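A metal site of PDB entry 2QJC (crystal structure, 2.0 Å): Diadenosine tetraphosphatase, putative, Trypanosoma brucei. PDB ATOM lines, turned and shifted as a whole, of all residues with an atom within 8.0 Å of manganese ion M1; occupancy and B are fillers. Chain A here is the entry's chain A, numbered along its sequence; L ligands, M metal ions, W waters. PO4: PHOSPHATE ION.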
ATOM      1  N   GLY A  25      25.944  -7.578  -0.528  1.00  0.00           N
ATOM      2  CA  GLY A  25      25.115  -7.381   0.648  1.00  0.00           C
ATOM      3  C   GLY A  25      24.537  -8.655   1.235  1.00  0.00           C
ATOM      4  O   GLY A  25      24.863  -9.762   0.783  1.00  0.00           O
ATOM      5  N   ASP A  26      23.669  -8.511   2.234  1.00  0.00           N
ATOM      6  CA  ASP A  26      23.074  -9.664   2.919  1.00  0.00           C
ATOM      7  C   ASP A  26      22.456 -10.673   1.949  1.00  0.00           C
ATOM      8  O   ASP A  26      21.522 -10.355   1.224  1.00  0.00           O
ATOM      9  CB  ASP A  26      22.010  -9.180   3.931  1.00  0.00           C
ATOM     10  CG  ASP A  26      22.598  -8.293   5.037  1.00  0.00           C
ATOM     11  OD1 ASP A  26      23.385  -7.374   4.717  1.00  0.00           O
ATOM     12  OD2 ASP A  26      22.258  -8.511   6.225  1.00  0.00           O
ATOM     13  N   ILE A  27      22.990 -11.895   1.958  1.00  0.00           N
ATOM     14  CA  ILE A  27      22.497 -12.961   1.072  1.00  0.00           C
ATOM     15  C   ILE A  27      21.347 -13.770   1.691  1.00  0.00           C
ATOM     16  O   ILE A  27      20.358 -14.079   1.015  1.00  0.00           O
ATOM     17  CB  ILE A  27      23.657 -13.911   0.677  1.00  0.00           C
ATOM     18  CG1 ILE A  27      24.721 -13.128  -0.096  1.00  0.00           C
ATOM     19  CG2 ILE A  27      23.124 -15.020  -0.206  1.00  0.00           C
ATOM     20  CD1 ILE A  27      26.045 -13.865  -0.266  1.00  0.00           C
ATOM     21  N   HIS A  28      21.459 -14.101   2.975  1.00  0.00           N
ATOM     22  CA  HIS A  28      20.408 -14.840   3.657  1.00  0.00           C
ATOM     23  C   HIS A  28      19.851 -16.027   2.868  1.00  0.00           C
ATOM     24  O   HIS A  28      18.660 -16.078   2.558  1.00  0.00           O
ATOM     25  CB  HIS A  28      19.247 -13.891   4.032  1.00  0.00           C
ATOM     26  CG  HIS A  28      19.485 -13.129   5.301  1.00  0.00           C
ATOM     27  ND1 HIS A  28      19.711 -13.741   6.506  1.00  0.00           N
ATOM     28  CD2 HIS A  28      19.499 -11.796   5.547  1.00  0.00           C
ATOM     29  CE1 HIS A  28      19.853 -12.822   7.446  1.00  0.00           C
ATOM     30  NE2 HIS A  28      19.728 -11.627   6.893  1.00  0.00           N
ATOM     31  N   VAL A  53      29.284  -9.386   3.079  1.00  0.00           N
ATOM     32  CA  VAL A  53      29.173  -8.576   4.288  1.00  0.00           C
ATOM     33  C   VAL A  53      28.617  -9.413   5.464  1.00  0.00           C
ATOM     34  O   VAL A  53      28.406  -8.912   6.566  1.00  0.00           O
ATOM     35  CB  VAL A  53      28.251  -7.348   4.090  1.00  0.00           C
ATOM     36  CG1 VAL A  53      28.806  -6.459   2.963  1.00  0.00           C
ATOM     37  CG2 VAL A  53      26.816  -7.787   3.815  1.00  0.00           C
ATOM     38  N   GLY A  54      28.393 -10.701   5.219  1.00  0.00           N
ATOM     39  CA  GLY A  54      27.887 -11.556   6.282  1.00  0.00           C
ATOM     40  C   GLY A  54      26.397 -11.791   6.185  1.00  0.00           C
ATOM     41  O   GLY A  54      25.726 -11.216   5.328  1.00  0.00           O
ATOM     42  N   ASP A  55      25.871 -12.612   7.088  1.00  0.00           N
ATOM     43  CA  ASP A  55      24.448 -12.951   7.100  1.00  0.00           C
ATOM     44  C   ASP A  55      24.220 -13.782   5.851  1.00  0.00           C
ATOM     45  O   ASP A  55      23.383 -13.471   5.001  1.00  0.00           O
ATOM     46  CB  ASP A  55      23.578 -11.676   7.089  1.00  0.00           C
ATOM     47  CG  ASP A  55      23.068 -11.306   8.472  1.00  0.00           C
ATOM     48  OD1 ASP A  55      23.651 -11.790   9.472  1.00  0.00           O
ATOM     49  OD2 ASP A  55      22.101 -10.524   8.569  1.00  0.00           O
ATOM     50  N   LEU A  56      24.987 -14.858   5.753  1.00  0.00           N
ATOM     51  CA  LEU A  56      24.920 -15.789   4.638  1.00  0.00           C
ATOM     52  C   LEU A  56      23.749 -16.753   4.771  1.00  0.00           C
ATOM     53  O   LEU A  56      23.250 -17.294   3.772  1.00  0.00           O
ATOM     54  CB  LEU A  56      26.221 -16.604   4.593  1.00  0.00           C
ATOM     55  CG  LEU A  56      27.500 -15.804   4.788  1.00  0.00           C
ATOM     56  CD1 LEU A  56      28.697 -16.741   4.701  1.00  0.00           C
ATOM     57  CD2 LEU A  56      27.583 -14.692   3.733  1.00  0.00           C
ATOM     58  N   VAL A  57      23.304 -16.958   6.005  1.00  0.00           N
ATOM     59  CA  VAL A  57      22.220 -17.896   6.293  1.00  0.00           C
ATOM     60  C   VAL A  57      20.923 -17.315   6.855  1.00  0.00           C
ATOM     61  O   VAL A  57      20.778 -16.098   7.044  1.00  0.00           O
ATOM     62  CB  VAL A  57      22.713 -18.965   7.283  1.00  0.00           C
ATOM     63  CG1 VAL A  57      24.094 -19.481   6.854  1.00  0.00           C
ATOM     64  CG2 VAL A  57      22.790 -18.382   8.686  1.00  0.00           C
ATOM     65  N   ASN A  58      19.984 -18.224   7.114  1.00  0.00           N
ATOM     66  CA  ASN A  58      18.676 -17.904   7.683  1.00  0.00           C
ATOM     67  C   ASN A  58      17.757 -17.128   6.736  1.00  0.00           C
ATOM     68  O   ASN A  58      18.219 -16.366   5.878  1.00  0.00           O
ATOM     69  CB  ASN A  58      18.863 -17.136   8.996  1.00  0.00           C
ATOM     70  CG  ASN A  58      17.654 -17.242   9.921  1.00  0.00           C
ATOM     71  OD1 ASN A  58      16.942 -18.247   9.908  1.00  0.00           O
ATOM     72  ND2 ASN A  58      17.446 -16.214  10.729  1.00  0.00           N
ATOM     73  N   LYS A  59      16.450 -17.362   6.898  1.00  0.00           N
ATOM     74  CA  LYS A  59      15.393 -16.726   6.123  1.00  0.00           C
ATOM     75  C   LYS A  59      15.236 -17.218   4.681  1.00  0.00           C
ATOM     76  O   LYS A  59      14.120 -17.498   4.233  1.00  0.00           O
ATOM     77  CB  LYS A  59      15.555 -15.199   6.105  1.00  0.00           C
ATOM     78  CG  LYS A  59      15.871 -14.550   7.463  1.00  0.00           C
ATOM     79  CD  LYS A  59      15.248 -15.292   8.640  1.00  0.00           C
ATOM     80  CE  LYS A  59      13.718 -15.339   8.571  1.00  0.00           C
ATOM     81  NZ  LYS A  59      13.144 -16.026   9.774  1.00  0.00           N
ATOM     82  N   GLY A  80      28.335 -12.167  10.079  1.00  0.00           N
ATOM     83  CA  GLY A  80      27.104 -11.414  10.302  1.00  0.00           C
ATOM     84  C   GLY A  80      26.502 -11.817  11.640  1.00  0.00           C
ATOM     85  O   GLY A  80      26.953 -12.786  12.239  1.00  0.00           O
ATOM     86  N   ASN A  81      25.485 -11.096  12.133  1.00  0.00           N
ATOM     87  CA  ASN A  81      24.941 -11.493  13.427  1.00  0.00           C
ATOM     88  C   ASN A  81      24.061 -12.732  13.370  1.00  0.00           C
ATOM     89  O   ASN A  81      23.874 -13.396  14.389  1.00  0.00           O
ATOM     90  CB  ASN A  81      24.200 -10.332  14.123  1.00  0.00           C
ATOM     91  CG  ASN A  81      23.011  -9.857  13.339  1.00  0.00           C
ATOM     92  OD1 ASN A  81      21.910  -9.730  13.891  1.00  0.00           O
ATOM     93  ND2 ASN A  81      23.213  -9.575  12.057  1.00  0.00           N
ATOM     94  N   HIS A  82      23.520 -13.047  12.197  1.00  0.00           N
ATOM     95  CA  HIS A  82      22.720 -14.253  12.064  1.00  0.00           C
ATOM     96  C   HIS A  82      23.662 -15.436  11.968  1.00  0.00           C
ATOM     97  O   HIS A  82      23.350 -16.534  12.445  1.00  0.00           O
ATOM     98  CB  HIS A  82      21.828 -14.178  10.822  1.00  0.00           C
ATOM     99  CG  HIS A  82      20.563 -13.414  11.047  1.00  0.00           C
ATOM    100  ND1 HIS A  82      19.396 -14.022  11.451  1.00  0.00           N
ATOM    101  CD2 HIS A  82      20.286 -12.091  10.930  1.00  0.00           C
ATOM    102  CE1 HIS A  82      18.447 -13.110  11.574  1.00  0.00           C
ATOM    103  NE2 HIS A  82      18.966 -11.932  11.264  1.00  0.00           N
ATOM    104  N   HIS A 141      30.076  -6.065   9.092  1.00  0.00           N
ATOM    105  CA  HIS A 141      28.674  -6.421   8.872  1.00  0.00           C
ATOM    106  C   HIS A 141      27.660  -5.288   9.084  1.00  0.00           C
ATOM    107  O   HIS A 141      26.810  -5.052   8.206  1.00  0.00           O
ATOM    108  CB  HIS A 141      28.274  -7.633   9.738  1.00  0.00           C
ATOM    109  CG  HIS A 141      26.831  -8.011   9.601  1.00  0.00           C
ATOM    110  ND1 HIS A 141      26.294  -8.459   8.412  1.00  0.00           N
ATOM    111  CD2 HIS A 141      25.803  -7.922  10.471  1.00  0.00           C
ATOM    112  CE1 HIS A 141      24.992  -8.640   8.563  1.00  0.00           C
ATOM    113  NE2 HIS A 141      24.662  -8.315   9.796  1.00  0.00           N
ATOM    114  N   THR A 159      28.604  -6.016  14.578  1.00  0.00           N
ATOM    115  CA  THR A 159      27.668  -6.922  13.934  1.00  0.00           C
ATOM    116  C   THR A 159      26.187  -6.560  14.102  1.00  0.00           C
ATOM    117  O   THR A 159      25.331  -7.185  13.476  1.00  0.00           O
ATOM    118  CB  THR A 159      27.843  -8.394  14.412  1.00  0.00           C
ATOM    119  OG1 THR A 159      27.703  -8.451  15.834  1.00  0.00           O
ATOM    120  CG2 THR A 159      29.206  -8.915  14.004  1.00  0.00           C
ATOM    121  N   ARG A 162      23.010   0.099  14.441  1.00  0.00           N
ATOM    122  CA  ARG A 162      22.179   0.816  13.480  1.00  0.00           C
ATOM    123  C   ARG A 162      22.274   2.317  13.767  1.00  0.00           C
ATOM    124  O   ARG A 162      22.308   3.148  12.853  1.00  0.00           O
ATOM    125  CB  ARG A 162      20.716   0.383  13.597  1.00  0.00           C
ATOM    126  CG  ARG A 162      20.420  -1.030  13.149  1.00  0.00           C
ATOM    127  CD  ARG A 162      18.999  -1.438  13.543  1.00  0.00           C
ATOM    128  NE  ARG A 162      18.829  -2.884  13.609  1.00  0.00           N
ATOM    129  CZ  ARG A 162      18.599  -3.662  12.560  1.00  0.00           C
ATOM    130  NH1 ARG A 162      18.521  -3.134  11.349  1.00  0.00           N
ATOM    131  NH2 ARG A 162      18.451  -4.977  12.722  1.00  0.00           N
ATOM    132  N   GLY A 203      26.319  -3.999   5.442  1.00  0.00           N
ATOM    133  CA  GLY A 203      24.963  -4.468   5.143  1.00  0.00           C
ATOM    134  C   GLY A 203      24.131  -4.384   6.422  1.00  0.00           C
ATOM    135  O   GLY A 203      23.971  -3.293   6.975  1.00  0.00           O
ATOM    136  N   HIS A 204      23.584  -5.506   6.863  1.00  0.00           N
ATOM    137  CA  HIS A 204      22.797  -5.597   8.114  1.00  0.00           C
ATOM    138  C   HIS A 204      21.460  -4.853   8.264  1.00  0.00           C
ATOM    139  O   HIS A 204      20.435  -5.475   8.570  1.00  0.00           O
ATOM    140  CB  HIS A 204      23.697  -5.224   9.294  1.00  0.00           C
ATOM    141  CG  HIS A 204      22.991  -5.210  10.628  1.00  0.00           C
ATOM    142  ND1 HIS A 204      22.399  -6.332  11.162  1.00  0.00           N
ATOM    143  CD2 HIS A 204      22.824  -4.231  11.535  1.00  0.00           C
ATOM    144  CE1 HIS A 204      21.887  -6.037  12.347  1.00  0.00           C
ATOM    145  NE2 HIS A 204      22.136  -4.763  12.601  1.00  0.00           N
ATOM    146  N   ASP A 205      21.481  -3.532   8.079  1.00  0.00           N
ATOM    147  CA  ASP A 205      20.311  -2.670   8.266  1.00  0.00           C
ATOM    148  C   ASP A 205      19.260  -2.668   7.146  1.00  0.00           C
ATOM    149  O   ASP A 205      19.064  -1.660   6.470  1.00  0.00           O
ATOM    150  CB  ASP A 205      20.804  -1.225   8.522  1.00  0.00           C
ATOM    151  CG  ASP A 205      19.752  -0.336   9.202  1.00  0.00           C
ATOM    152  OD1 ASP A 205      20.071   0.843   9.485  1.00  0.00           O
ATOM    153  OD2 ASP A 205      18.616  -0.792   9.451  1.00  0.00           O
ATOM    154  N   ALA A 206      18.582  -3.800   6.963  1.00  0.00           N
ATOM    155  CA  ALA A 206      17.554  -3.937   5.925  1.00  0.00           C
ATOM    156  C   ALA A 206      16.451  -2.880   6.053  1.00  0.00           C
ATOM    157  O   ALA A 206      15.875  -2.456   5.054  1.00  0.00           O
ATOM    158  CB  ALA A 206      16.926  -5.343   5.987  1.00  0.00           C
ATOM    159  N   ASP A 222      22.625  -3.364   2.156  1.00  0.00           N
ATOM    160  CA  ASP A 222      21.483  -4.246   2.435  1.00  0.00           C
ATOM    161  C   ASP A 222      20.167  -3.763   1.819  1.00  0.00           C
ATOM    162  O   ASP A 222      19.352  -3.131   2.492  1.00  0.00           O
ATOM    163  CB  ASP A 222      21.300  -4.470   3.935  1.00  0.00           C
ATOM    164  CG  ASP A 222      20.373  -5.645   4.219  1.00  0.00           C
ATOM    165  OD1 ASP A 222      19.781  -6.180   3.245  1.00  0.00           O
ATOM    166  OD2 ASP A 222      20.236  -6.035   5.399  1.00  0.00           O
ATOM    167  N   ARG A 224      17.658  -5.529   1.009  1.00  0.00           N
ATOM    168  CA  ARG A 224      16.577  -6.466   1.356  1.00  0.00           C
ATOM    169  C   ARG A 224      16.314  -7.626   0.409  1.00  0.00           C
ATOM    170  O   ARG A 224      15.162  -7.986   0.195  1.00  0.00           O
ATOM    171  CB  ARG A 224      15.257  -5.707   1.515  1.00  0.00           C
ATOM    172  CG  ARG A 224      15.379  -4.341   2.115  1.00  0.00           C
ATOM    173  CD  ARG A 224      14.208  -3.474   1.680  1.00  0.00           C
ATOM    174  NE  ARG A 224      13.863  -2.564   2.760  1.00  0.00           N
ATOM    175  CZ  ARG A 224      12.732  -2.599   3.438  1.00  0.00           C
ATOM    176  NH1 ARG A 224      11.795  -3.492   3.145  1.00  0.00           N
ATOM    177  NH2 ARG A 224      12.560  -1.766   4.450  1.00  0.00           N
ATOM    178  N   VAL A 226      16.367 -10.959   0.580  1.00  0.00           N
ATOM    179  CA  VAL A 226      15.496 -12.014   1.108  1.00  0.00           C
ATOM    180  C   VAL A 226      14.060 -11.597   1.402  1.00  0.00           C
ATOM    181  O   VAL A 226      13.175 -12.441   1.486  1.00  0.00           O
ATOM    182  CB  VAL A 226      16.084 -12.639   2.392  1.00  0.00           C
ATOM    183  CG1 VAL A 226      16.028 -11.628   3.542  1.00  0.00           C
ATOM    184  CG2 VAL A 226      15.325 -13.913   2.749  1.00  0.00           C
ATOM    185  N   TYR A 227      13.829 -10.300   1.554  1.00  0.00           N
ATOM    186  CA  TYR A 227      12.490  -9.784   1.840  1.00  0.00           C
ATOM    187  C   TYR A 227      11.766  -9.383   0.549  1.00  0.00           C
ATOM    188  O   TYR A 227      10.703  -8.752   0.606  1.00  0.00           O
ATOM    189  CB  TYR A 227      12.581  -8.569   2.756  1.00  0.00           C
ATOM    190  CG  TYR A 227      13.255  -8.817   4.085  1.00  0.00           C
ATOM    191  CD1 TYR A 227      12.593  -9.488   5.123  1.00  0.00           C
ATOM    192  CD2 TYR A 227      14.537  -8.317   4.338  1.00  0.00           C
ATOM    193  CE1 TYR A 227      13.186  -9.646   6.375  1.00  0.00           C
ATOM    194  CE2 TYR A 227      15.139  -8.473   5.569  1.00  0.00           C
ATOM    195  CZ  TYR A 227      14.470  -9.125   6.587  1.00  0.00           C
ATOM    196  OH  TYR A 227      15.080  -9.236   7.816  1.00  0.00           O
HETATM  197  P   PO4 L   1      18.675  -8.290  10.027  1.00  0.00           P
HETATM  198  O1  PO4 L   1      17.747  -8.142   8.705  1.00  0.00           O
HETATM  199  O2  PO4 L   1      18.868  -6.841  10.640  1.00  0.00           O
HETATM  200  O3  PO4 L   1      17.948  -9.227  11.035  1.00  0.00           O
HETATM  201  O4  PO4 L   1      20.062  -8.866   9.599  1.00  0.00           O
HETATM  202 MN    MN M   1      20.669  -9.424   7.493  1.00  0.00          MN
HETATM  203 MN    MN M   2      22.421  -8.511  10.454  1.00  0.00          MN
HETATM  204  O   HOH W   1      19.099  -8.237   6.413  1.00  0.00           O
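The backbone NH (N) of His 82 sits at hydrogen-bond distance from the side-chain carboxylate (OD1) of Asp 55, 3.0 Å away. The backbone NH (N) of Asn 81 sits at hydrogen-bond distance from the side-chain carboxylate (OD1) of Asp 55, at 3.3 Å. The backbone NH (N) of Ile 27 lies within hydrogen-bond range of the backbone carbonyl oxygen (O) of Asp 55, at 3.4 Å. The side-chain carboxylate (OD1) of Asp 26 is in hydrogen-bond range of the backbone NH (N) of His 204 (2.9 Å). A ring nitrogen (ND1) of His 28 sits at hydrogen-bond distance from the backbone carbonyl oxygen of Val 57, at 2.6 Å. The backbone carbonyl oxygen of Asn 58 lies within hydrogen-bond range of a ring nitrogen (ND1) of His 28, at 3.1 Å.
Of the 25 residues printed, 3 come within 4 Å of manganese ion M1.
Manganese ion M1 is bound by OD2 of Asp 55 (2.1 Å). Manganese ion M1 is bound by the side-chain carboxylate (OD2) of Asp 26, at 2.2 Å. Manganese ion M1 is bound by water W1 (2.2 Å). Manganese ion M1 is bound by an oxygen (O4) of the ligand (2.3 Å). Manganese ion M1 is bound by NE2 of His 28 (2.5 Å).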
